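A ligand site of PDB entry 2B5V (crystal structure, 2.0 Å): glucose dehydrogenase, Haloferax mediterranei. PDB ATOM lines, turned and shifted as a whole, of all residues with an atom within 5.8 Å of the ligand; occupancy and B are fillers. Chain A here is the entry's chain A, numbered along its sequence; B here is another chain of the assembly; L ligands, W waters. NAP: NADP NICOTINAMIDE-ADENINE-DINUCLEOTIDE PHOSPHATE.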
ATOM      1  N   ASP A  38      10.824  -2.075 -26.496  1.00  0.00           N
ATOM      2  CA  ASP A  38      12.032  -2.801 -26.833  1.00  0.00           C
ATOM      3  C   ASP A  38      11.969  -3.471 -28.214  1.00  0.00           C
ATOM      4  O   ASP A  38      10.908  -3.504 -28.848  1.00  0.00           O
ATOM      5  CB  ASP A  38      12.246  -3.867 -25.756  1.00  0.00           C
ATOM      6  CG  ASP A  38      13.618  -4.453 -25.789  1.00  0.00           C
ATOM      7  OD1 ASP A  38      14.581  -3.672 -25.892  1.00  0.00           O
ATOM      8  OD2 ASP A  38      13.703  -5.679 -25.688  1.00  0.00           O
ATOM      9  N   GLY A  39      13.098  -4.025 -28.641  1.00  0.00           N
ATOM     10  CA  GLY A  39      13.154  -4.728 -29.914  1.00  0.00           C
ATOM     11  C   GLY A  39      12.136  -5.851 -30.044  1.00  0.00           C
ATOM     12  O   GLY A  39      11.500  -6.011 -31.089  1.00  0.00           O
ATOM     13  N   THR A  40      11.935  -6.632 -28.981  1.00  0.00           N
ATOM     14  CA  THR A  40      10.980  -7.732 -29.045  1.00  0.00           C
ATOM     15  C   THR A  40       9.597  -7.184 -29.390  1.00  0.00           C
ATOM     16  O   THR A  40       8.878  -7.756 -30.198  1.00  0.00           O
ATOM     17  CB  THR A  40      10.908  -8.483 -27.689  1.00  0.00           C
ATOM     18  OG1 THR A  40      10.350  -7.617 -26.688  1.00  0.00           O
ATOM     19  CG2 THR A  40      12.319  -8.936 -27.253  1.00  0.00           C
ATOM     20  N   GLU A  43       9.434  -6.783 -32.897  1.00  0.00           N
ATOM     21  CA  GLU A  43       9.347  -8.079 -33.566  1.00  0.00           C
ATOM     22  C   GLU A  43       7.872  -8.494 -33.651  1.00  0.00           C
ATOM     23  O   GLU A  43       7.397  -8.909 -34.713  1.00  0.00           O
ATOM     24  CB  GLU A  43      10.106  -9.147 -32.783  1.00  0.00           C
ATOM     25  CG  GLU A  43      11.402  -9.585 -33.437  1.00  0.00           C
ATOM     26  CD  GLU A  43      12.527  -8.593 -33.262  1.00  0.00           C
ATOM     27  OE1 GLU A  43      12.347  -7.411 -33.657  1.00  0.00           O
ATOM     28  OE2 GLU A  43      13.591  -8.988 -32.735  1.00  0.00           O
ATOM     29  N   ILE A 154      19.189  -7.812 -17.015  1.00  0.00           N
ATOM     30  CA  ILE A 154      19.720  -8.711 -18.032  1.00  0.00           C
ATOM     31  C   ILE A 154      21.257  -8.738 -17.926  1.00  0.00           C
ATOM     32  O   ILE A 154      21.875  -9.803 -17.829  1.00  0.00           O
ATOM     33  CB  ILE A 154      19.248  -8.241 -19.454  1.00  0.00           C
ATOM     34  CG1 ILE A 154      17.704  -8.364 -19.568  1.00  0.00           C
ATOM     35  CG2 ILE A 154      19.917  -9.083 -20.531  1.00  0.00           C
ATOM     36  CD1 ILE A 154      17.149  -9.713 -19.148  1.00  0.00           C
ATOM     37  N   LEU A 179      29.695  -5.198 -28.122  1.00  0.00           N
ATOM     38  CA  LEU A 179      29.320  -5.257 -29.527  1.00  0.00           C
ATOM     39  C   LEU A 179      27.842  -4.835 -29.616  1.00  0.00           C
ATOM     40  O   LEU A 179      26.971  -5.507 -29.054  1.00  0.00           O
ATOM     41  CB  LEU A 179      29.482  -6.667 -30.067  1.00  0.00           C
ATOM     42  CG  LEU A 179      30.766  -7.376 -29.615  1.00  0.00           C
ATOM     43  CD1 LEU A 179      30.831  -8.749 -30.254  1.00  0.00           C
ATOM     44  CD2 LEU A 179      31.988  -6.541 -30.044  1.00  0.00           C
ATOM     45  N   GLY A 180      27.561  -3.724 -30.312  1.00  0.00           N
ATOM     46  CA  GLY A 180      26.169  -3.293 -30.447  1.00  0.00           C
ATOM     47  C   GLY A 180      25.944  -1.980 -29.746  1.00  0.00           C
ATOM     48  O   GLY A 180      26.297  -1.814 -28.569  1.00  0.00           O
ATOM     49  N   ASN A 181      25.323  -1.032 -30.455  1.00  0.00           N
ATOM     50  CA  ASN A 181      25.072   0.281 -29.894  1.00  0.00           C
ATOM     51  C   ASN A 181      23.576   0.522 -29.697  1.00  0.00           C
ATOM     52  O   ASN A 181      23.106   1.652 -29.805  1.00  0.00           O
ATOM     53  CB  ASN A 181      25.698   1.351 -30.807  1.00  0.00           C
ATOM     54  CG  ASN A 181      25.209   1.261 -32.234  1.00  0.00           C
ATOM     55  OD1 ASN A 181      25.076   0.169 -32.796  1.00  0.00           O
ATOM     56  ND2 ASN A 181      24.945   2.413 -32.824  1.00  0.00           N
ATOM     57  N   GLY A 182      22.853  -0.548 -29.412  1.00  0.00           N
ATOM     58  CA  GLY A 182      21.406  -0.439 -29.137  1.00  0.00           C
ATOM     59  C   GLY A 182      21.262  -0.127 -27.650  1.00  0.00           C
ATOM     60  O   GLY A 182      22.267   0.029 -26.962  1.00  0.00           O
ATOM     61  N   SER A 183      20.019  -0.038 -27.161  1.00  0.00           N
ATOM     62  CA  SER A 183      19.719   0.260 -25.756  1.00  0.00           C
ATOM     63  C   SER A 183      20.476  -0.654 -24.784  1.00  0.00           C
ATOM     64  O   SER A 183      21.046  -0.178 -23.811  1.00  0.00           O
ATOM     65  CB  SER A 183      18.192   0.094 -25.496  1.00  0.00           C
ATOM     66  OG  SER A 183      17.428   0.848 -26.415  1.00  0.00           O
ATOM     67  N   LEU A 184      20.471  -1.959 -25.034  1.00  0.00           N
ATOM     68  CA  LEU A 184      21.147  -2.909 -24.156  1.00  0.00           C
ATOM     69  C   LEU A 184      22.662  -2.728 -24.185  1.00  0.00           C
ATOM     70  O   LEU A 184      23.303  -2.734 -23.138  1.00  0.00           O
ATOM     71  CB  LEU A 184      20.813  -4.375 -24.550  1.00  0.00           C
ATOM     72  CG  LEU A 184      21.350  -5.467 -23.595  1.00  0.00           C
ATOM     73  CD1 LEU A 184      20.777  -5.237 -22.222  1.00  0.00           C
ATOM     74  CD2 LEU A 184      21.003  -6.910 -24.090  1.00  0.00           C
ATOM     75  N   GLY A 185      23.258  -2.593 -25.376  1.00  0.00           N
ATOM     76  CA  GLY A 185      24.697  -2.381 -25.464  1.00  0.00           C
ATOM     77  C   GLY A 185      25.175  -1.082 -24.773  1.00  0.00           C
ATOM     78  O   GLY A 185      26.180  -1.084 -24.073  1.00  0.00           O
ATOM     79  N   LEU A 205      31.262  -1.404 -30.421  1.00  0.00           N
ATOM     80  CA  LEU A 205      31.065  -1.669 -31.838  1.00  0.00           C
ATOM     81  C   LEU A 205      29.718  -1.203 -32.388  1.00  0.00           C
ATOM     82  O   LEU A 205      28.657  -1.507 -31.807  1.00  0.00           O
ATOM     83  CB  LEU A 205      31.170  -3.190 -32.096  1.00  0.00           C
ATOM     84  CG  LEU A 205      31.311  -3.601 -33.566  1.00  0.00           C
ATOM     85  CD1 LEU A 205      32.780  -3.530 -33.966  1.00  0.00           C
ATOM     86  CD2 LEU A 205      30.764  -4.999 -33.795  1.00  0.00           C
ATOM     87  N   GLY A 206      29.756  -0.476 -33.510  1.00  0.00           N
ATOM     88  CA  GLY A 206      28.523  -0.008 -34.146  1.00  0.00           C
ATOM     89  C   GLY A 206      28.816   0.098 -35.643  1.00  0.00           C
ATOM     90  O   GLY A 206      29.906  -0.277 -36.092  1.00  0.00           O
ATOM     91  N   ARG A 207      27.876   0.616 -36.415  1.00  0.00           N
ATOM     92  CA  ARG A 207      28.096   0.785 -37.844  1.00  0.00           C
ATOM     93  C   ARG A 207      27.328   2.031 -38.339  1.00  0.00           C
ATOM     94  O   ARG A 207      26.647   1.974 -39.369  1.00  0.00           O
ATOM     95  CB  ARG A 207      27.633  -0.470 -38.590  1.00  0.00           C
ATOM     96  CG  ARG A 207      26.185  -0.826 -38.349  1.00  0.00           C
ATOM     97  CD  ARG A 207      25.797  -2.103 -39.096  1.00  0.00           C
ATOM     98  NE  ARG A 207      24.409  -2.452 -38.809  1.00  0.00           N
ATOM     99  CZ  ARG A 207      23.820  -3.583 -39.208  1.00  0.00           C
ATOM    100  NH1 ARG A 207      24.497  -4.476 -39.930  1.00  0.00           N
ATOM    101  NH2 ARG A 207      22.574  -3.843 -38.852  1.00  0.00           N
ATOM    102  N   ARG A 208      27.436   3.115 -37.574  1.00  0.00           N
ATOM    103  CA  ARG A 208      26.764   4.388 -37.885  1.00  0.00           C
ATOM    104  C   ARG A 208      27.750   5.434 -38.380  1.00  0.00           C
ATOM    105  O   ARG A 208      28.928   5.403 -37.997  1.00  0.00           O
ATOM    106  CB  ARG A 208      26.107   4.991 -36.629  1.00  0.00           C
ATOM    107  CG  ARG A 208      25.053   4.128 -35.904  1.00  0.00           C
ATOM    108  CD  ARG A 208      23.772   4.020 -36.713  1.00  0.00           C
ATOM    109  NE  ARG A 208      22.743   3.219 -36.045  1.00  0.00           N
ATOM    110  CZ  ARG A 208      21.962   3.662 -35.072  1.00  0.00           C
ATOM    111  NH1 ARG A 208      22.057   4.917 -34.621  1.00  0.00           N
ATOM    112  NH2 ARG A 208      21.054   2.841 -34.557  1.00  0.00           N
ATOM    113  N   SER A 228      32.292  -1.219 -37.347  1.00  0.00           N
ATOM    114  CA  SER A 228      32.519  -2.548 -37.896  1.00  0.00           C
ATOM    115  C   SER A 228      32.710  -2.562 -39.419  1.00  0.00           C
ATOM    116  O   SER A 228      33.209  -3.545 -39.977  1.00  0.00           O
ATOM    117  CB  SER A 228      31.378  -3.487 -37.483  1.00  0.00           C
ATOM    118  OG  SER A 228      30.153  -3.133 -38.090  1.00  0.00           O
ATOM    119  N   GLU A 248      28.450  -9.399 -26.256  1.00  0.00           N
ATOM    120  CA  GLU A 248      27.789  -9.394 -27.533  1.00  0.00           C
ATOM    121  C   GLU A 248      26.306  -9.063 -27.435  1.00  0.00           C
ATOM    122  O   GLU A 248      25.523  -9.806 -26.831  1.00  0.00           O
ATOM    123  CB  GLU A 248      28.006 -10.749 -28.230  1.00  0.00           C
ATOM    124  CG  GLU A 248      27.302 -10.923 -29.582  1.00  0.00           C
ATOM    125  CD  GLU A 248      25.837 -11.272 -29.462  1.00  0.00           C
ATOM    126  OE1 GLU A 248      25.513 -12.175 -28.655  1.00  0.00           O
ATOM    127  OE2 GLU A 248      25.001 -10.668 -30.185  1.00  0.00           O
ATOM    128  N   ALA A 249      25.916  -7.937 -28.017  1.00  0.00           N
ATOM    129  CA  ALA A 249      24.520  -7.550 -27.997  1.00  0.00           C
ATOM    130  C   ALA A 249      24.094  -7.036 -29.394  1.00  0.00           C
ATOM    131  O   ALA A 249      23.456  -5.997 -29.497  1.00  0.00           O
ATOM    132  CB  ALA A 249      24.282  -6.484 -26.925  1.00  0.00           C
ATOM    133  N   THR A 250      24.474  -7.772 -30.437  1.00  0.00           N
ATOM    134  CA  THR A 250      24.112  -7.382 -31.797  1.00  0.00           C
ATOM    135  C   THR A 250      23.144  -8.348 -32.434  1.00  0.00           C
ATOM    136  O   THR A 250      22.351  -7.952 -33.294  1.00  0.00           O
ATOM    137  CB  THR A 250      25.324  -7.294 -32.730  1.00  0.00           C
ATOM    138  OG1 THR A 250      25.992  -8.574 -32.770  1.00  0.00           O
ATOM    139  CG2 THR A 250      26.292  -6.262 -32.249  1.00  0.00           C
ATOM    140  N   GLY A 251      23.195  -9.608 -32.037  1.00  0.00           N
ATOM    141  CA  GLY A 251      22.318 -10.594 -32.635  1.00  0.00           C
ATOM    142  C   GLY A 251      22.880 -11.037 -33.990  1.00  0.00           C
ATOM    143  O   GLY A 251      22.189 -11.696 -34.743  1.00  0.00           O
ATOM    144  N   PHE A 252      24.149 -10.709 -34.261  1.00  0.00           N
ATOM    145  CA  PHE A 252      24.815 -11.075 -35.517  1.00  0.00           C
ATOM    146  C   PHE A 252      25.712 -12.292 -35.250  1.00  0.00           C
ATOM    147  O   PHE A 252      26.768 -12.164 -34.613  1.00  0.00           O
ATOM    148  CB  PHE A 252      25.642  -9.883 -35.996  1.00  0.00           C
ATOM    149  CG  PHE A 252      26.161 -10.005 -37.405  1.00  0.00           C
ATOM    150  CD1 PHE A 252      25.299 -10.262 -38.472  1.00  0.00           C
ATOM    151  CD2 PHE A 252      27.512  -9.778 -37.681  1.00  0.00           C
ATOM    152  CE1 PHE A 252      25.771 -10.303 -39.794  1.00  0.00           C
ATOM    153  CE2 PHE A 252      28.001  -9.808 -39.005  1.00  0.00           C
ATOM    154  CZ  PHE A 252      27.122 -10.076 -40.061  1.00  0.00           C
ATOM    155  N   HIS A 255      29.572 -12.442 -35.144  1.00  0.00           N
ATOM    156  CA  HIS A 255      30.185 -11.889 -33.938  1.00  0.00           C
ATOM    157  C   HIS A 255      30.441 -12.924 -32.845  1.00  0.00           C
ATOM    158  O   HIS A 255      31.464 -12.867 -32.171  1.00  0.00           O
ATOM    159  CB  HIS A 255      29.331 -10.760 -33.367  1.00  0.00           C
ATOM    160  CG  HIS A 255      29.328  -9.526 -34.215  1.00  0.00           C
ATOM    161  ND1 HIS A 255      30.284  -9.264 -35.170  1.00  0.00           N
ATOM    162  CD2 HIS A 255      28.489  -8.464 -34.221  1.00  0.00           C
ATOM    163  CE1 HIS A 255      30.042  -8.083 -35.723  1.00  0.00           C
ATOM    164  NE2 HIS A 255      28.949  -7.583 -35.173  1.00  0.00           N
ATOM    165  N   LEU A 271      27.417 -13.919 -24.475  1.00  0.00           N
ATOM    166  CA  LEU A 271      26.555 -13.768 -25.645  1.00  0.00           C
ATOM    167  C   LEU A 271      25.114 -13.500 -25.182  1.00  0.00           C
ATOM    168  O   LEU A 271      24.578 -14.232 -24.349  1.00  0.00           O
ATOM    169  CB  LEU A 271      26.579 -15.057 -26.499  1.00  0.00           C
ATOM    170  CG  LEU A 271      28.000 -15.472 -26.950  1.00  0.00           C
ATOM    171  CD1 LEU A 271      27.940 -16.754 -27.731  1.00  0.00           C
ATOM    172  CD2 LEU A 271      28.616 -14.382 -27.814  1.00  0.00           C
ATOM    173  N   LEU A 272      24.514 -12.431 -25.700  1.00  0.00           N
ATOM    174  CA  LEU A 272      23.142 -12.085 -25.347  1.00  0.00           C
ATOM    175  C   LEU A 272      22.240 -12.025 -26.578  1.00  0.00           C
ATOM    176  O   LEU A 272      21.012 -11.992 -26.467  1.00  0.00           O
ATOM    177  CB  LEU A 272      23.088 -10.702 -24.649  1.00  0.00           C
ATOM    178  CG  LEU A 272      23.520 -10.504 -23.177  1.00  0.00           C
ATOM    179  CD1 LEU A 272      22.494 -11.169 -22.268  1.00  0.00           C
ATOM    180  CD2 LEU A 272      24.943 -11.053 -22.924  1.00  0.00           C
ATOM    181  N   GLY A 273      22.845 -11.956 -27.764  1.00  0.00           N
ATOM    182  CA  GLY A 273      22.059 -11.814 -28.976  1.00  0.00           C
ATOM    183  C   GLY A 273      21.222 -13.008 -29.379  1.00  0.00           C
ATOM    184  O   GLY A 273      21.596 -14.135 -29.097  1.00  0.00           O
ATOM    185  N   VAL A 274      20.088 -12.776 -30.031  1.00  0.00           N
ATOM    186  CA  VAL A 274      19.236 -13.883 -30.460  1.00  0.00           C
ATOM    187  C   VAL A 274      19.027 -13.845 -31.980  1.00  0.00           C
ATOM    188  O   VAL A 274      18.085 -13.229 -32.449  1.00  0.00           O
ATOM    189  CB  VAL A 274      17.898 -13.838 -29.763  1.00  0.00           C
ATOM    190  CG1 VAL A 274      17.144 -15.148 -29.991  1.00  0.00           C
ATOM    191  CG2 VAL A 274      18.110 -13.584 -28.276  1.00  0.00           C
ATOM    192  N   PRO A 275      19.896 -14.510 -32.749  1.00  0.00           N
ATOM    193  CA  PRO A 275      19.810 -14.554 -34.208  1.00  0.00           C
ATOM    194  C   PRO A 275      19.012 -15.750 -34.713  1.00  0.00           C
ATOM    195  O   PRO A 275      18.763 -16.702 -33.976  1.00  0.00           O
ATOM    196  CB  PRO A 275      21.262 -14.690 -34.621  1.00  0.00           C
ATOM    197  CG  PRO A 275      21.746 -15.730 -33.597  1.00  0.00           C
ATOM    198  CD  PRO A 275      21.090 -15.245 -32.282  1.00  0.00           C
ATOM    199  N   SER A 301      23.537 -16.128 -22.008  1.00  0.00           N
ATOM    200  CA  SER A 301      22.686 -15.773 -20.865  1.00  0.00           C
ATOM    201  C   SER A 301      21.375 -15.196 -21.395  1.00  0.00           C
ATOM    202  O   SER A 301      21.371 -14.481 -22.404  1.00  0.00           O
ATOM    203  CB  SER A 301      23.377 -14.706 -19.983  1.00  0.00           C
ATOM    204  OG  SER A 301      22.620 -14.396 -18.820  1.00  0.00           O
ATOM    205  N   VAL A 302      20.268 -15.491 -20.722  1.00  0.00           N
ATOM    206  CA  VAL A 302      18.981 -14.952 -21.150  1.00  0.00           C
ATOM    207  C   VAL A 302      18.166 -14.654 -19.913  1.00  0.00           C
ATOM    208  O   VAL A 302      18.314 -15.329 -18.883  1.00  0.00           O
ATOM    209  CB  VAL A 302      18.193 -15.955 -22.082  1.00  0.00           C
ATOM    210  CG1 VAL A 302      17.904 -17.274 -21.335  1.00  0.00           C
ATOM    211  CG2 VAL A 302      16.887 -15.321 -22.527  1.00  0.00           C
ATOM    212  N   ASN A 303      17.346 -13.593 -19.980  1.00  0.00           N
ATOM    213  CA  ASN A 303      16.440 -13.255 -18.893  1.00  0.00           C
ATOM    214  C   ASN A 303      17.187 -12.920 -17.596  1.00  0.00           C
ATOM    215  O   ASN A 303      18.368 -12.605 -17.621  1.00  0.00           O
ATOM    216  CB  ASN A 303      15.494 -14.433 -18.681  1.00  0.00           C
ATOM    217  CG  ASN A 303      14.212 -14.043 -17.963  1.00  0.00           C
ATOM    218  OD1 ASN A 303      13.384 -13.266 -18.499  1.00  0.00           O
ATOM    219  ND2 ASN A 303      14.020 -14.569 -16.759  1.00  0.00           N
ATOM    220  N   ASP A 345      17.445   6.058 -36.488  1.00  0.00           N
ATOM    221  CA  ASP A 345      18.766   6.148 -35.890  1.00  0.00           C
ATOM    222  C   ASP A 345      18.879   7.074 -34.691  1.00  0.00           C
ATOM    223  O   ASP A 345      19.718   6.844 -33.806  1.00  0.00           O
ATOM    224  CB  ASP A 345      19.803   6.583 -36.932  1.00  0.00           C
ATOM    225  CG  ASP A 345      20.167   5.476 -37.876  1.00  0.00           C
ATOM    226  OD1 ASP A 345      21.051   5.716 -38.736  1.00  0.00           O
ATOM    227  OD2 ASP A 345      19.598   4.370 -37.775  1.00  0.00           O
ATOM    228  N   VAL B 292      22.676 -18.861 -26.287  1.00  0.00           N
ATOM    229  CA  VAL B 292      21.975 -17.837 -25.523  1.00  0.00           C
ATOM    230  C   VAL B 292      20.670 -18.258 -24.892  1.00  0.00           C
ATOM    231  O   VAL B 292      20.516 -18.148 -23.679  1.00  0.00           O
ATOM    232  CB  VAL B 292      21.723 -16.581 -26.392  1.00  0.00           C
ATOM    233  CG1 VAL B 292      20.984 -15.496 -25.571  1.00  0.00           C
ATOM    234  CG2 VAL B 292      23.080 -16.046 -26.924  1.00  0.00           C
ATOM    235  N   LEU B 293      19.730 -18.739 -25.697  1.00  0.00           N
ATOM    236  CA  LEU B 293      18.426 -19.104 -25.161  1.00  0.00           C
ATOM    237  C   LEU B 293      18.452 -20.240 -24.140  1.00  0.00           C
ATOM    238  O   LEU B 293      17.517 -20.399 -23.365  1.00  0.00           O
ATOM    239  CB  LEU B 293      17.478 -19.497 -26.314  1.00  0.00           C
ATOM    240  CG  LEU B 293      17.110 -18.312 -27.244  1.00  0.00           C
ATOM    241  CD1 LEU B 293      16.034 -18.771 -28.176  1.00  0.00           C
ATOM    242  CD2 LEU B 293      16.624 -17.100 -26.433  1.00  0.00           C
HETATM  243  PA  NAP L   1      18.816  -3.474 -31.029  1.00  0.00           P
HETATM  244  O1A NAP L   1      18.486  -4.136 -32.228  1.00  0.00           O
HETATM  245  O2A NAP L   1      18.152  -2.262 -30.432  1.00  0.00           O
HETATM  246  O5B NAP L   1      20.335  -3.072 -31.086  1.00  0.00           O
HETATM  247  C5B NAP L   1      21.296  -3.959 -31.721  1.00  0.00           C
HETATM  248  C4B NAP L   1      22.299  -2.901 -32.218  1.00  0.00           C
HETATM  249  O4B NAP L   1      23.449  -3.583 -32.837  1.00  0.00           O
HETATM  250  C3B NAP L   1      21.795  -1.916 -33.336  1.00  0.00           C
HETATM  251  O3B NAP L   1      22.114  -0.616 -32.889  1.00  0.00           O
HETATM  252  C2B NAP L   1      22.550  -2.343 -34.601  1.00  0.00           C
HETATM  253  O2B NAP L   1      22.968  -1.280 -35.454  1.00  0.00           O
HETATM  254  C1B NAP L   1      23.794  -3.051 -34.057  1.00  0.00           C
HETATM  255  N9A NAP L   1      24.308  -4.006 -35.009  1.00  0.00           N
HETATM  256  C8A NAP L   1      23.749  -5.103 -35.623  1.00  0.00           C
HETATM  257  N7A NAP L   1      24.575  -5.715 -36.454  1.00  0.00           N
HETATM  258  C5A NAP L   1      25.738  -4.970 -36.382  1.00  0.00           C
HETATM  259  C6A NAP L   1      26.949  -5.126 -37.044  1.00  0.00           C
HETATM  260  N6A NAP L   1      27.257  -6.076 -37.958  1.00  0.00           N
HETATM  261  N1A NAP L   1      27.949  -4.203 -36.757  1.00  0.00           N
HETATM  262  C2A NAP L   1      27.740  -3.183 -35.834  1.00  0.00           C
HETATM  263  N3A NAP L   1      26.540  -3.008 -35.173  1.00  0.00           N
HETATM  264  C4A NAP L   1      25.578  -3.918 -35.473  1.00  0.00           C
HETATM  265  O3  NAP L   1      18.791  -4.491 -29.815  1.00  0.00           O
HETATM  266  PN  NAP L   1      18.857  -4.187 -28.235  1.00  0.00           P
HETATM  267  O1N NAP L   1      20.117  -3.516 -27.809  1.00  0.00           O
HETATM  268  O2N NAP L   1      17.665  -4.071 -27.409  1.00  0.00           O
HETATM  269  O5D NAP L   1      19.169  -5.769 -28.427  1.00  0.00           O
HETATM  270  C5D NAP L   1      20.522  -6.297 -28.755  1.00  0.00           C
HETATM  271  C4D NAP L   1      20.421  -7.823 -28.923  1.00  0.00           C
HETATM  272  O4D NAP L   1      20.201  -8.435 -27.612  1.00  0.00           O
HETATM  273  C3D NAP L   1      19.232  -8.395 -29.812  1.00  0.00           C
HETATM  274  O3D NAP L   1      19.640  -9.514 -30.636  1.00  0.00           O
HETATM  275  C2D NAP L   1      18.202  -8.826 -28.790  1.00  0.00           C
HETATM  276  O2D NAP L   1      17.372  -9.849 -29.297  1.00  0.00           O
HETATM  277  C1D NAP L   1      19.062  -9.323 -27.704  1.00  0.00           C
HETATM  278  N1N NAP L   1      18.540  -9.400 -26.341  1.00  0.00           N
HETATM  279  C2N NAP L   1      18.776 -10.537 -25.560  1.00  0.00           C
HETATM  280  C3N NAP L   1      18.285 -10.584 -24.290  1.00  0.00           C
HETATM  281  C7N NAP L   1      18.572 -11.843 -23.462  1.00  0.00           C
HETATM  282  O7N NAP L   1      18.085 -11.883 -22.354  1.00  0.00           O
HETATM  283  N7N NAP L   1      19.310 -12.827 -23.939  1.00  0.00           N
HETATM  284  C4N NAP L   1      17.507  -9.477 -23.730  1.00  0.00           C
HETATM  285  C5N NAP L   1      17.292  -8.339 -24.542  1.00  0.00           C
HETATM  286  C6N NAP L   1      17.808  -8.265 -25.865  1.00  0.00           C
HETATM  287  P2B NAP L   1      22.033  -0.595 -36.612  1.00  0.00           P
HETATM  288  O1X NAP L   1      20.891   0.075 -35.871  1.00  0.00           O
HETATM  289  O2X NAP L   1      23.019   0.349 -37.209  1.00  0.00           O
HETATM  290  O3X NAP L   1      21.567  -1.725 -37.498  1.00  0.00           O
HETATM  291  O   HOH W   1      16.934  -4.869 -24.635  1.00  0.00           O
HETATM  292  O   HOH W   2      15.619  -6.815 -27.269  1.00  0.00           O
HETATM  293  O   HOH W   3      16.568  -1.835 -33.479  1.00  0.00           O
HETATM  294  O   HOH W   4      25.136   0.705 -35.431  1.00  0.00           O
HETATM  295  O   HOH W   5      14.343  -8.223 -24.785  1.00  0.00           O
HETATM  296  O   HOH W   6      30.188  -6.753 -39.005  1.00  0.00           O
HETATM  297  O   HOH W   7      22.721  -3.360 -28.335  1.00  0.00           O
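The backbone NH of Asn 303 is in hydrogen-bond range of an oxygen (O7N) of the ligand (3.0 Å). A nitrogen (N7N) of the ligand sits close to the backbone carbonyl oxygen of Leu 272, at 3.2 Å. N of Val 274 sits at hydrogen-bond distance from O3D of the ligand. OG of Ser 228 lies within hydrogen-bond range of N1A of the ligand, 2.8 Å away. The backbone carbonyl oxygen (O) of Ser 301 sits at hydrogen-bond distance from a nitrogen (N7N) of the ligand. O1X of the ligand is in salt-bridge range of NH2 of Arg 208, at 3.1 Å. The side-chain amide oxygen of Asn 181 is in hydrogen-bond range of an oxygen (O3B) of the ligand (3.1 Å). An oxygen (O3X) of the ligand lies within salt-bridge range of the guanidinium group (NH2) of Arg 207. The backbone NH (N) of Leu 184 lies within hydrogen-bond range of an oxygen (O1N) of the ligand, at 3.2 Å.
The backbone NH of Gly 251 is in hydrogen-bond range of the side-chain carboxylate of Glu 248 (2.8 Å). The backbone NH (N) of Leu 272 lies within hydrogen-bond range of the backbone carbonyl oxygen (O) of Glu 248, 3.0 Å away. The backbone NH (N) of Gly 273 is in hydrogen-bond range of the side-chain carboxylate (OE1) of Glu 248, 2.8 Å away. The backbone NH (N) of Phe 252 lies close to the side-chain hydroxyl (OG1) of Thr 250 (3.2 Å). OE2 of Glu 248 sits at hydrogen-bond distance from N of Thr 250 (3.0 Å). The backbone NH of Ala 249 sits at hydrogen-bond distance from the backbone carbonyl oxygen of Leu 179 (2.8 Å). OD2 of Asp 345 is in salt-bridge range of NE of Arg 208, 3.8 Å away. The backbone carbonyl oxygen of Leu 205 lies within hydrogen-bond range of the backbone NH of Gly 180 (2.9 Å).
An oxygen (O2N) of the ligand sits close to the side-chain carboxylate (OD1) of Asp 38. Ile 154 touches the ligand. Gly 180 touches the ligand. Gly 182 touches the ligand. N of Ser 183 touches O1N of the ligand, at 3.5 Å. Gly 206 touches the ligand. Ala 249 touches the ligand (O to C5D, 3.0 Å). Thr 250 touches the ligand (O to C8A, 3.9 Å). CA of Gly 251 touches O3D of the ligand, 3.5 Å away. CD2 of Phe 252 touches N6A of the ligand, 3.7 Å away. His 255 touches the ligand (NE2 to N6A, 3.6 Å). CA of Gly 273 touches O3D of the ligand, 3.7 Å away. CA of Val 302 touches O7N of the ligand, 3.4 Å away. Val 292 of chain B touches the ligand. Hydrophobic or aromatic side chains within 4 Å of the ligand: Ile 154, Leu 184, Phe 252, Leu 272, Val 274, Val 302 and Val 292 of chain B. Within 4 Å of the ligand: Asp 38, Ile 154, Gly 180, Asn 181, Gly 182, Ser 183, Leu 184, Gly 206, Arg 207, Arg 208, Ser 228, Ala 249, Thr 250, Gly 251, Phe 252, His 255, Leu 272, Gly 273, Val 274, Ser 301, Val 302, Asn 303 and Val 292 of chain B.
Water W7 lies within hydrogen-bond range of an oxygen (O1N) of the ligand (2.7 Å), the backbone carbonyl oxygen (O) of Ala 249 (3.0 Å), the backbone NH (N) of Gly 182 (3.0 Å) and the backbone NH (N) of Gly 185 (3.1 Å). Water W4 lies within hydrogen-bond range of OD1 of Asn 181 (2.7 Å), O2X of the ligand (2.8 Å) and N of Arg 207 (2.9 Å). Water W2 lies within hydrogen-bond range of OD2 of Asp 38 and O2N of the ligand. Water W1 lies within hydrogen-bond range of the side-chain carboxylate (OD1) of Asp 38 (2.9 Å) and an oxygen (O2N) of the ligand (3.0 Å).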
